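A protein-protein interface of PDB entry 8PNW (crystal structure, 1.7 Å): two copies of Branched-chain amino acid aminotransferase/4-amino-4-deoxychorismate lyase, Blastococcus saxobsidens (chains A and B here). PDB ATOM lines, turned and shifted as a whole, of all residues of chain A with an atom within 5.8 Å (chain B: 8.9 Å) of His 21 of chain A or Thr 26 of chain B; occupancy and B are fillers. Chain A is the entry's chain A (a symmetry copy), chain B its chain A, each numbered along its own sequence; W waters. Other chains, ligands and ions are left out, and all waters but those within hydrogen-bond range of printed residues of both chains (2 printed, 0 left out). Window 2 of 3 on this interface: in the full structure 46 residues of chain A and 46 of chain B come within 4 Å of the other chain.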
ATOM      1  N   ARG A   5     -17.493 -21.515   1.346  1.00  0.00           N
ATOM      2  CA  ARG A   5     -16.325 -22.039   0.636  1.00  0.00           C
ATOM      3  C   ARG A   5     -15.117 -21.333   1.240  1.00  0.00           C
ATOM      4  O   ARG A   5     -15.243 -20.208   1.754  1.00  0.00           O
ATOM      5  CB  ARG A   5     -16.479 -21.817  -0.868  1.00  0.00           C
ATOM      6  CG  ARG A   5     -17.614 -22.593  -1.508  1.00  0.00           C
ATOM      7  CD  ARG A   5     -17.765 -22.231  -2.989  1.00  0.00           C
ATOM      8  NE  ARG A   5     -17.799 -20.767  -3.137  1.00  0.00           N
ATOM      9  CZ  ARG A   5     -17.553 -20.077  -4.251  1.00  0.00           C
ATOM     10  NH1 ARG A   5     -17.241 -20.688  -5.390  1.00  0.00           N
ATOM     11  NH2 ARG A   5     -17.580 -18.749  -4.201  1.00  0.00           N
ATOM     12  N   PRO A  19     -10.883 -14.656  -0.031  1.00  0.00           N
ATOM     13  CA  PRO A  19     -12.289 -14.982  -0.234  1.00  0.00           C
ATOM     14  C   PRO A  19     -12.498 -15.933  -1.427  1.00  0.00           C
ATOM     15  O   PRO A  19     -11.849 -15.775  -2.468  1.00  0.00           O
ATOM     16  CB  PRO A  19     -12.997 -13.640  -0.445  1.00  0.00           C
ATOM     17  CG  PRO A  19     -11.940 -12.557  -0.193  1.00  0.00           C
ATOM     18  CD  PRO A  19     -10.591 -13.220  -0.020  1.00  0.00           C
ATOM     19  N   ALA A  20     -13.422 -16.884  -1.266  1.00  0.00           N
ATOM     20  CA  ALA A  20     -13.684 -17.967  -2.234  1.00  0.00           C
ATOM     21  C   ALA A  20     -14.120 -17.394  -3.590  1.00  0.00           C
ATOM     22  O   ALA A  20     -13.875 -18.050  -4.602  1.00  0.00           O
ATOM     23  CB  ALA A  20     -14.689 -18.931  -1.645  1.00  0.00           C
ATOM     24  N   HIS A  21     -14.737 -16.211  -3.628  1.00  0.00           N
ATOM     25  CA  HIS A  21     -15.257 -15.569  -4.876  1.00  0.00           C
ATOM     26  C   HIS A  21     -14.144 -14.778  -5.576  1.00  0.00           C
ATOM     27  O   HIS A  21     -14.319 -14.389  -6.742  1.00  0.00           O
ATOM     28  CB  HIS A  21     -16.484 -14.688  -4.596  1.00  0.00           C
ATOM     29  CG  HIS A  21     -16.227 -13.589  -3.631  1.00  0.00           C
ATOM     30  ND1 HIS A  21     -15.720 -12.344  -4.032  1.00  0.00           N
ATOM     31  CD2 HIS A  21     -16.366 -13.546  -2.290  1.00  0.00           C
ATOM     32  CE1 HIS A  21     -15.558 -11.584  -2.967  1.00  0.00           C
ATOM     33  NE2 HIS A  21     -15.949 -12.307  -1.877  1.00  0.00           N
ATOM     34  N   GLN A  22     -13.018 -14.547  -4.918  1.00  0.00           N
ATOM     35  CA  GLN A  22     -11.954 -13.684  -5.473  1.00  0.00           C
ATOM     36  C   GLN A  22     -11.133 -14.495  -6.467  1.00  0.00           C
ATOM     37  O   GLN A  22     -10.686 -15.608  -6.170  1.00  0.00           O
ATOM     38  CB  GLN A  22     -11.048 -13.192  -4.359  1.00  0.00           C
ATOM     39  CG  GLN A  22      -9.917 -12.276  -4.817  1.00  0.00           C
ATOM     40  CD  GLN A  22      -9.295 -11.637  -3.599  1.00  0.00           C
ATOM     41  OE1 GLN A  22      -9.990 -10.998  -2.813  1.00  0.00           O
ATOM     42  NE2 GLN A  22      -8.008 -11.870  -3.397  1.00  0.00           N
ATOM     43  N   PRO A  23     -10.812 -13.936  -7.647  1.00  0.00           N
ATOM     44  CA  PRO A  23      -9.915 -14.626  -8.569  1.00  0.00           C
ATOM     45  C   PRO A  23      -8.569 -14.913  -7.921  1.00  0.00           C
ATOM     46  O   PRO A  23      -8.136 -14.050  -7.182  1.00  0.00           O
ATOM     47  CB  PRO A  23      -9.721 -13.629  -9.723  1.00  0.00           C
ATOM     48  CG  PRO A  23     -10.919 -12.717  -9.619  1.00  0.00           C
ATOM     49  CD  PRO A  23     -11.275 -12.634  -8.148  1.00  0.00           C
ATOM     50  N   VAL A  24      -7.946 -16.066  -8.227  1.00  0.00           N
ATOM     51  CA  VAL A  24      -6.614 -16.434  -7.676  1.00  0.00           C
ATOM     52  C   VAL A  24      -5.630 -16.867  -8.736  1.00  0.00           C
ATOM     53  O   VAL A  24      -4.471 -16.976  -8.374  1.00  0.00           O
ATOM     54  CB  VAL A  24      -6.726 -17.565  -6.632  1.00  0.00           C
ATOM     55  CG1 VAL A  24      -7.525 -17.106  -5.428  1.00  0.00           C
ATOM     56  CG2 VAL A  24      -7.311 -18.829  -7.260  1.00  0.00           C
ATOM     57  N   VAL A  25      -6.063 -17.215  -9.953  1.00  0.00           N
ATOM     58  CA  VAL A  25      -5.144 -17.649 -11.025  1.00  0.00           C
ATOM     59  C   VAL A  25      -5.212 -16.638 -12.184  1.00  0.00           C
ATOM     60  O   VAL A  25      -6.332 -16.198 -12.523  1.00  0.00           O
ATOM     61  CB  VAL A  25      -5.545 -19.084 -11.396  1.00  0.00           C
ATOM     62  CG1 VAL A  25      -5.161 -19.474 -12.789  1.00  0.00           C
ATOM     63  CG2 VAL A  25      -4.971 -20.067 -10.363  1.00  0.00           C
ATOM     64  N   ARG B  11     -17.565  -9.611 -18.939  1.00  0.00           N
ATOM     65  CA  ARG B  11     -18.201  -9.286 -17.635  1.00  0.00           C
ATOM     66  C   ARG B  11     -19.474  -8.474 -17.938  1.00  0.00           C
ATOM     67  O   ARG B  11     -19.356  -7.428 -18.567  1.00  0.00           O
ATOM     68  CB  ARG B  11     -17.132  -8.531 -16.842  1.00  0.00           C
ATOM     69  CG  ARG B  11     -17.338  -8.391 -15.343  1.00  0.00           C
ATOM     70  CD  ARG B  11     -16.062  -7.832 -14.700  1.00  0.00           C
ATOM     71  NE  ARG B  11     -15.014  -8.841 -14.501  1.00  0.00           N
ATOM     72  CZ  ARG B  11     -13.784  -8.594 -14.042  1.00  0.00           C
ATOM     73  NH1 ARG B  11     -13.421  -7.361 -13.727  1.00  0.00           N
ATOM     74  NH2 ARG B  11     -12.913  -9.581 -13.891  1.00  0.00           N
ATOM     75  N   PRO B  23      -4.984 -11.790 -11.079  1.00  0.00           N
ATOM     76  CA  PRO B  23      -5.787 -13.005 -11.187  1.00  0.00           C
ATOM     77  C   PRO B  23      -7.132 -12.723 -11.838  1.00  0.00           C
ATOM     78  O   PRO B  23      -7.660 -11.669 -11.540  1.00  0.00           O
ATOM     79  CB  PRO B  23      -6.009 -13.441  -9.730  1.00  0.00           C
ATOM     80  CG  PRO B  23      -4.889 -12.767  -8.975  1.00  0.00           C
ATOM     81  CD  PRO B  23      -4.602 -11.465  -9.697  1.00  0.00           C
ATOM     82  N   VAL B  24      -7.652 -13.654 -12.659  1.00  0.00           N
ATOM     83  CA  VAL B  24      -8.973 -13.496 -13.323  1.00  0.00           C
ATOM     84  C   VAL B  24      -9.877 -14.693 -13.145  1.00  0.00           C
ATOM     85  O   VAL B  24     -11.038 -14.538 -13.483  1.00  0.00           O
ATOM     86  CB  VAL B  24      -8.818 -13.231 -14.836  1.00  0.00           C
ATOM     87  CG1 VAL B  24      -8.108 -11.914 -15.079  1.00  0.00           C
ATOM     88  CG2 VAL B  24      -8.113 -14.398 -15.523  1.00  0.00           C
ATOM     89  N   VAL B  25      -9.368 -15.866 -12.751  1.00  0.00           N
ATOM     90  CA  VAL B  25     -10.206 -17.067 -12.564  1.00  0.00           C
ATOM     91  C   VAL B  25     -10.168 -17.480 -11.081  1.00  0.00           C
ATOM     92  O   VAL B  25      -9.071 -17.438 -10.482  1.00  0.00           O
ATOM     93  CB  VAL B  25      -9.682 -18.128 -13.543  1.00  0.00           C
ATOM     94  CG1 VAL B  25      -9.976 -19.533 -13.121  1.00  0.00           C
ATOM     95  CG2 VAL B  25     -10.221 -17.844 -14.954  1.00  0.00           C
ATOM     96  N   THR B  26     -11.315 -17.856 -10.521  1.00  0.00           N
ATOM     97  CA  THR B  26     -11.397 -18.292  -9.101  1.00  0.00           C
ATOM     98  C   THR B  26     -10.942 -19.745  -8.965  1.00  0.00           C
ATOM     99  O   THR B  26     -10.836 -20.468  -9.957  1.00  0.00           O
ATOM    100  CB  THR B  26     -12.797 -18.105  -8.500  1.00  0.00           C
ATOM    101  OG1 THR B  26     -13.624 -19.183  -8.942  1.00  0.00           O
ATOM    102  CG2 THR B  26     -13.427 -16.758  -8.839  1.00  0.00           C
ATOM    103  N   ALA B  27     -10.727 -20.186  -7.730  1.00  0.00           N
ATOM    104  CA  ALA B  27     -10.240 -21.548  -7.461  1.00  0.00           C
ATOM    105  C   ALA B  27     -11.258 -22.573  -7.918  1.00  0.00           C
ATOM    106  O   ALA B  27     -10.829 -23.745  -8.192  1.00  0.00           O
ATOM    107  CB  ALA B  27      -9.935 -21.716  -5.998  1.00  0.00           C
ATOM    108  N   PHE B  28     -12.534 -22.188  -8.015  1.00  0.00           N
ATOM    109  CA  PHE B  28     -13.635 -23.130  -8.287  1.00  0.00           C
ATOM    110  C   PHE B  28     -13.975 -23.149  -9.783  1.00  0.00           C
ATOM    111  O   PHE B  28     -14.906 -23.866 -10.153  1.00  0.00           O
ATOM    112  CB  PHE B  28     -14.838 -22.810  -7.403  1.00  0.00           C
ATOM    113  CG  PHE B  28     -14.567 -23.080  -5.954  1.00  0.00           C
ATOM    114  CD1 PHE B  28     -14.688 -24.370  -5.469  1.00  0.00           C
ATOM    115  CD2 PHE B  28     -14.168 -22.074  -5.108  1.00  0.00           C
ATOM    116  CE1 PHE B  28     -14.431 -24.655  -4.141  1.00  0.00           C
ATOM    117  CE2 PHE B  28     -13.881 -22.366  -3.785  1.00  0.00           C
ATOM    118  CZ  PHE B  28     -13.973 -23.656  -3.325  1.00  0.00           C
ATOM    119  N   ASP B  29     -13.240 -22.412 -10.616  1.00  0.00           N
ATOM    120  CA  ASP B  29     -13.522 -22.411 -12.078  1.00  0.00           C
ATOM    121  C   ASP B  29     -13.204 -23.801 -12.619  1.00  0.00           C
ATOM    122  O   ASP B  29     -12.113 -24.314 -12.362  1.00  0.00           O
ATOM    123  CB  ASP B  29     -12.736 -21.336 -12.803  1.00  0.00           C
ATOM    124  CG  ASP B  29     -13.321 -21.028 -14.159  1.00  0.00           C
ATOM    125  OD1 ASP B  29     -13.247 -21.901 -15.028  1.00  0.00           O
ATOM    126  OD2 ASP B  29     -13.751 -19.886 -14.320  1.00  0.00           O
ATOM    127  N   LEU B  30     -14.141 -24.390 -13.329  1.00  0.00           N
ATOM    128  CA  LEU B  30     -13.971 -25.756 -13.863  1.00  0.00           C
ATOM    129  C   LEU B  30     -12.898 -25.783 -14.958  1.00  0.00           C
ATOM    130  O   LEU B  30     -12.431 -26.849 -15.272  1.00  0.00           O
ATOM    131  CB  LEU B  30     -15.333 -26.207 -14.355  1.00  0.00           C
ATOM    132  CG  LEU B  30     -16.288 -26.652 -13.254  1.00  0.00           C
ATOM    133  CD1 LEU B  30     -17.676 -26.847 -13.837  1.00  0.00           C
ATOM    134  CD2 LEU B  30     -15.786 -27.937 -12.589  1.00  0.00           C
ATOM    135  N   GLY B  31     -12.554 -24.646 -15.554  1.00  0.00           N
ATOM    136  CA  GLY B  31     -11.481 -24.589 -16.553  1.00  0.00           C
ATOM    137  C   GLY B  31     -10.142 -24.896 -15.910  1.00  0.00           C
ATOM    138  O   GLY B  31      -9.279 -25.447 -16.583  1.00  0.00           O
ATOM    139  N   LEU B  32      -9.973 -24.470 -14.658  1.00  0.00           N
ATOM    140  CA  LEU B  32      -8.765 -24.757 -13.854  1.00  0.00           C
ATOM    141  C   LEU B  32      -8.874 -26.174 -13.288  1.00  0.00           C
ATOM    142  O   LEU B  32      -7.910 -26.947 -13.437  1.00  0.00           O
ATOM    143  CB  LEU B  32      -8.678 -23.719 -12.732  1.00  0.00           C
ATOM    144  CG  LEU B  32      -7.549 -23.927 -11.744  1.00  0.00           C
ATOM    145  CD1 LEU B  32      -6.212 -23.969 -12.467  1.00  0.00           C
ATOM    146  CD2 LEU B  32      -7.585 -22.877 -10.644  1.00  0.00           C
ATOM    147  N   GLY B  33      -9.940 -26.418 -12.534  1.00  0.00           N
ATOM    148  CA  GLY B  33     -10.059 -27.646 -11.711  1.00  0.00           C
ATOM    149  C   GLY B  33     -10.200 -28.913 -12.522  1.00  0.00           C
ATOM    150  O   GLY B  33      -9.793 -29.983 -12.048  1.00  0.00           O
ATOM    151  N   THR B 100     -14.545 -21.368 -20.522  1.00  0.00           N
ATOM    152  CA  THR B 100     -14.647 -22.471 -19.529  1.00  0.00           C
ATOM    153  C   THR B 100     -16.084 -22.681 -19.070  1.00  0.00           C
ATOM    154  O   THR B 100     -16.930 -21.757 -19.206  1.00  0.00           O
ATOM    155  CB  THR B 100     -13.779 -22.240 -18.297  1.00  0.00           C
ATOM    156  OG1 THR B 100     -14.530 -21.521 -17.319  1.00  0.00           O
ATOM    157  CG2 THR B 100     -12.492 -21.523 -18.592  1.00  0.00           C
ATOM    158  N   GLY B 102     -16.998 -22.589 -16.258  1.00  0.00           N
ATOM    159  CA  GLY B 102     -17.208 -21.672 -15.120  1.00  0.00           C
ATOM    160  C   GLY B 102     -17.475 -22.422 -13.833  1.00  0.00           C
ATOM    161  O   GLY B 102     -16.790 -23.396 -13.590  1.00  0.00           O
ATOM    162  N   LEU B 103     -18.411 -21.960 -13.008  1.00  0.00           N
ATOM    163  CA  LEU B 103     -18.639 -22.609 -11.682  1.00  0.00           C
ATOM    164  C   LEU B 103     -19.499 -23.858 -11.842  1.00  0.00           C
ATOM    165  O   LEU B 103     -19.478 -24.642 -10.883  1.00  0.00           O
ATOM    166  CB  LEU B 103     -19.279 -21.630 -10.701  1.00  0.00           C
ATOM    167  CG  LEU B 103     -18.418 -20.450 -10.268  1.00  0.00           C
ATOM    168  CD1 LEU B 103     -19.196 -19.571  -9.286  1.00  0.00           C
ATOM    169  CD2 LEU B 103     -17.130 -20.905  -9.615  1.00  0.00           C
ATOM    170  N   THR B 110     -17.021 -18.844 -18.239  1.00  0.00           N
ATOM    171  CA  THR B 110     -15.962 -17.825 -18.147  1.00  0.00           C
ATOM    172  C   THR B 110     -15.398 -17.631 -19.553  1.00  0.00           C
ATOM    173  O   THR B 110     -15.031 -18.616 -20.216  1.00  0.00           O
ATOM    174  CB  THR B 110     -14.834 -18.289 -17.219  1.00  0.00           C
ATOM    175  OG1 THR B 110     -15.444 -18.625 -15.980  1.00  0.00           O
ATOM    176  CG2 THR B 110     -13.766 -17.244 -17.018  1.00  0.00           C
HETATM  177  O   HOH W   1     -11.110 -18.307  -5.435  1.00  0.00           O
HETATM  178  O   HOH W   2     -15.612 -18.935  -6.986  1.00  0.00           O
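Pro 23 of chain A touches its own counterpart, Pro 23 of chain B. Pro 23 of chain A touches Val 24 of chain B, and with the chains exchanged Val 24 of chain A touches Pro 23 of chain B. Pro 23 of chain A touches Val 25 of chain B, and with the chains exchanged Val 25 of chain A touches Pro 23 of chain B. Val 24 of chain A touches Val 25 of chain B, and with the chains exchanged Val 25 of chain A touches Val 24 of chain B. 3 positions are printed for both chains. Of the 14 pairs that touch across the chains among the printed residues, 8 have their exchanged pair printed and touching as well.
The backbone carbonyl oxygen (O) of Val 25 of chain A is in hydrogen-bond range of the backbone NH (N) of Val 24 of chain B. N of Val 24 of chain A sits at hydrogen-bond distance from O of Val 25 of chain B. N of Val 25 of chain B is in hydrogen-bond range of O of Val 25 of chain A, 3.1 Å away.
Water W2 lies within hydrogen-bond range of OG1 of Thr 26 of chain B (2.8 Å), NH1 of Arg 5 of chain A (2.9 Å) and O of Ala 20 of chain A (3.1 Å). Water W1 lies within hydrogen-bond range of the backbone carbonyl oxygen of Gln 22 of chain A (2.8 Å), the backbone carbonyl oxygen of Ala 20 of chain A (2.9 Å) and the backbone NH of Ala 27 of chain B (3.0 Å).
OG1 of Thr 26 of chain B sits close to N of Phe 28 of chain B, 3.3 Å away.
Among the printed residues, pairs that only touch across the chains: His 21 of chain A with Thr 26 of chain B, Pro 23 of chain A with Pro 23 of chain B, Arg 5 of chain A with Phe 28 of chain B, Val 25 of chain A with Pro 23 of chain B, Pro 23 of chain A with Val 25 of chain B, Pro 23 of chain A with Val 24 of chain B, Val 24 of chain A with Pro 23 of chain B, Val 24 of chain A with Ala 27 of chain B, Val 25 of chain A with Leu 32 of chain B, Pro 23 of chain A with Thr 26 of chain B and Gln 22 of chain A with Thr 26 of chain B.
No residue of chain B comes within 4 Å of Ala 20 of chain A. His 21 of chain A touches one residue of chain B. Printed residues of chain B within 4 Å of Pro 23 of chain A: Pro 23, Val 24, Val 25 and Thr 26. Of the printed residues of chain B, Val 24 of chain A touches Pro 23, Val 25 and Ala 27. Of the printed residues of chain A, Phe 28 of chain B touches Arg 5 (3.4 Å). Leu 103 of chain B touches none of the printed residues of chain A. The nearest printed residue of chain A that does not touch Thr 26 of chain B is Ala 20 of chain A (4.04 Å). The nearest printed residue of chain B that does not touch Arg 5 of chain A is Leu 103 of chain B (4.2 Å).
Of the 8 printed residues of chain A, 6 touch a printed residue of chain B. Printed residues of chain A that touch a printed residue of chain B: Arg 5, His 21, Gln 22, Pro 23, Val 24 and Val 25. Hydrophobic or aromatic side chains of chain A that line the printed part of chain B: Pro 23, Val 24 and Val 25. Along chain A the printed residues that touch a printed residue of chain B span positions 5 to 25. Among the printed residues, 14 pairs touch across the chains. Among the printed residues, no Asp or Glu carboxylate lies within 4 Å of a Lys or Arg side-chain nitrogen of the other chain.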
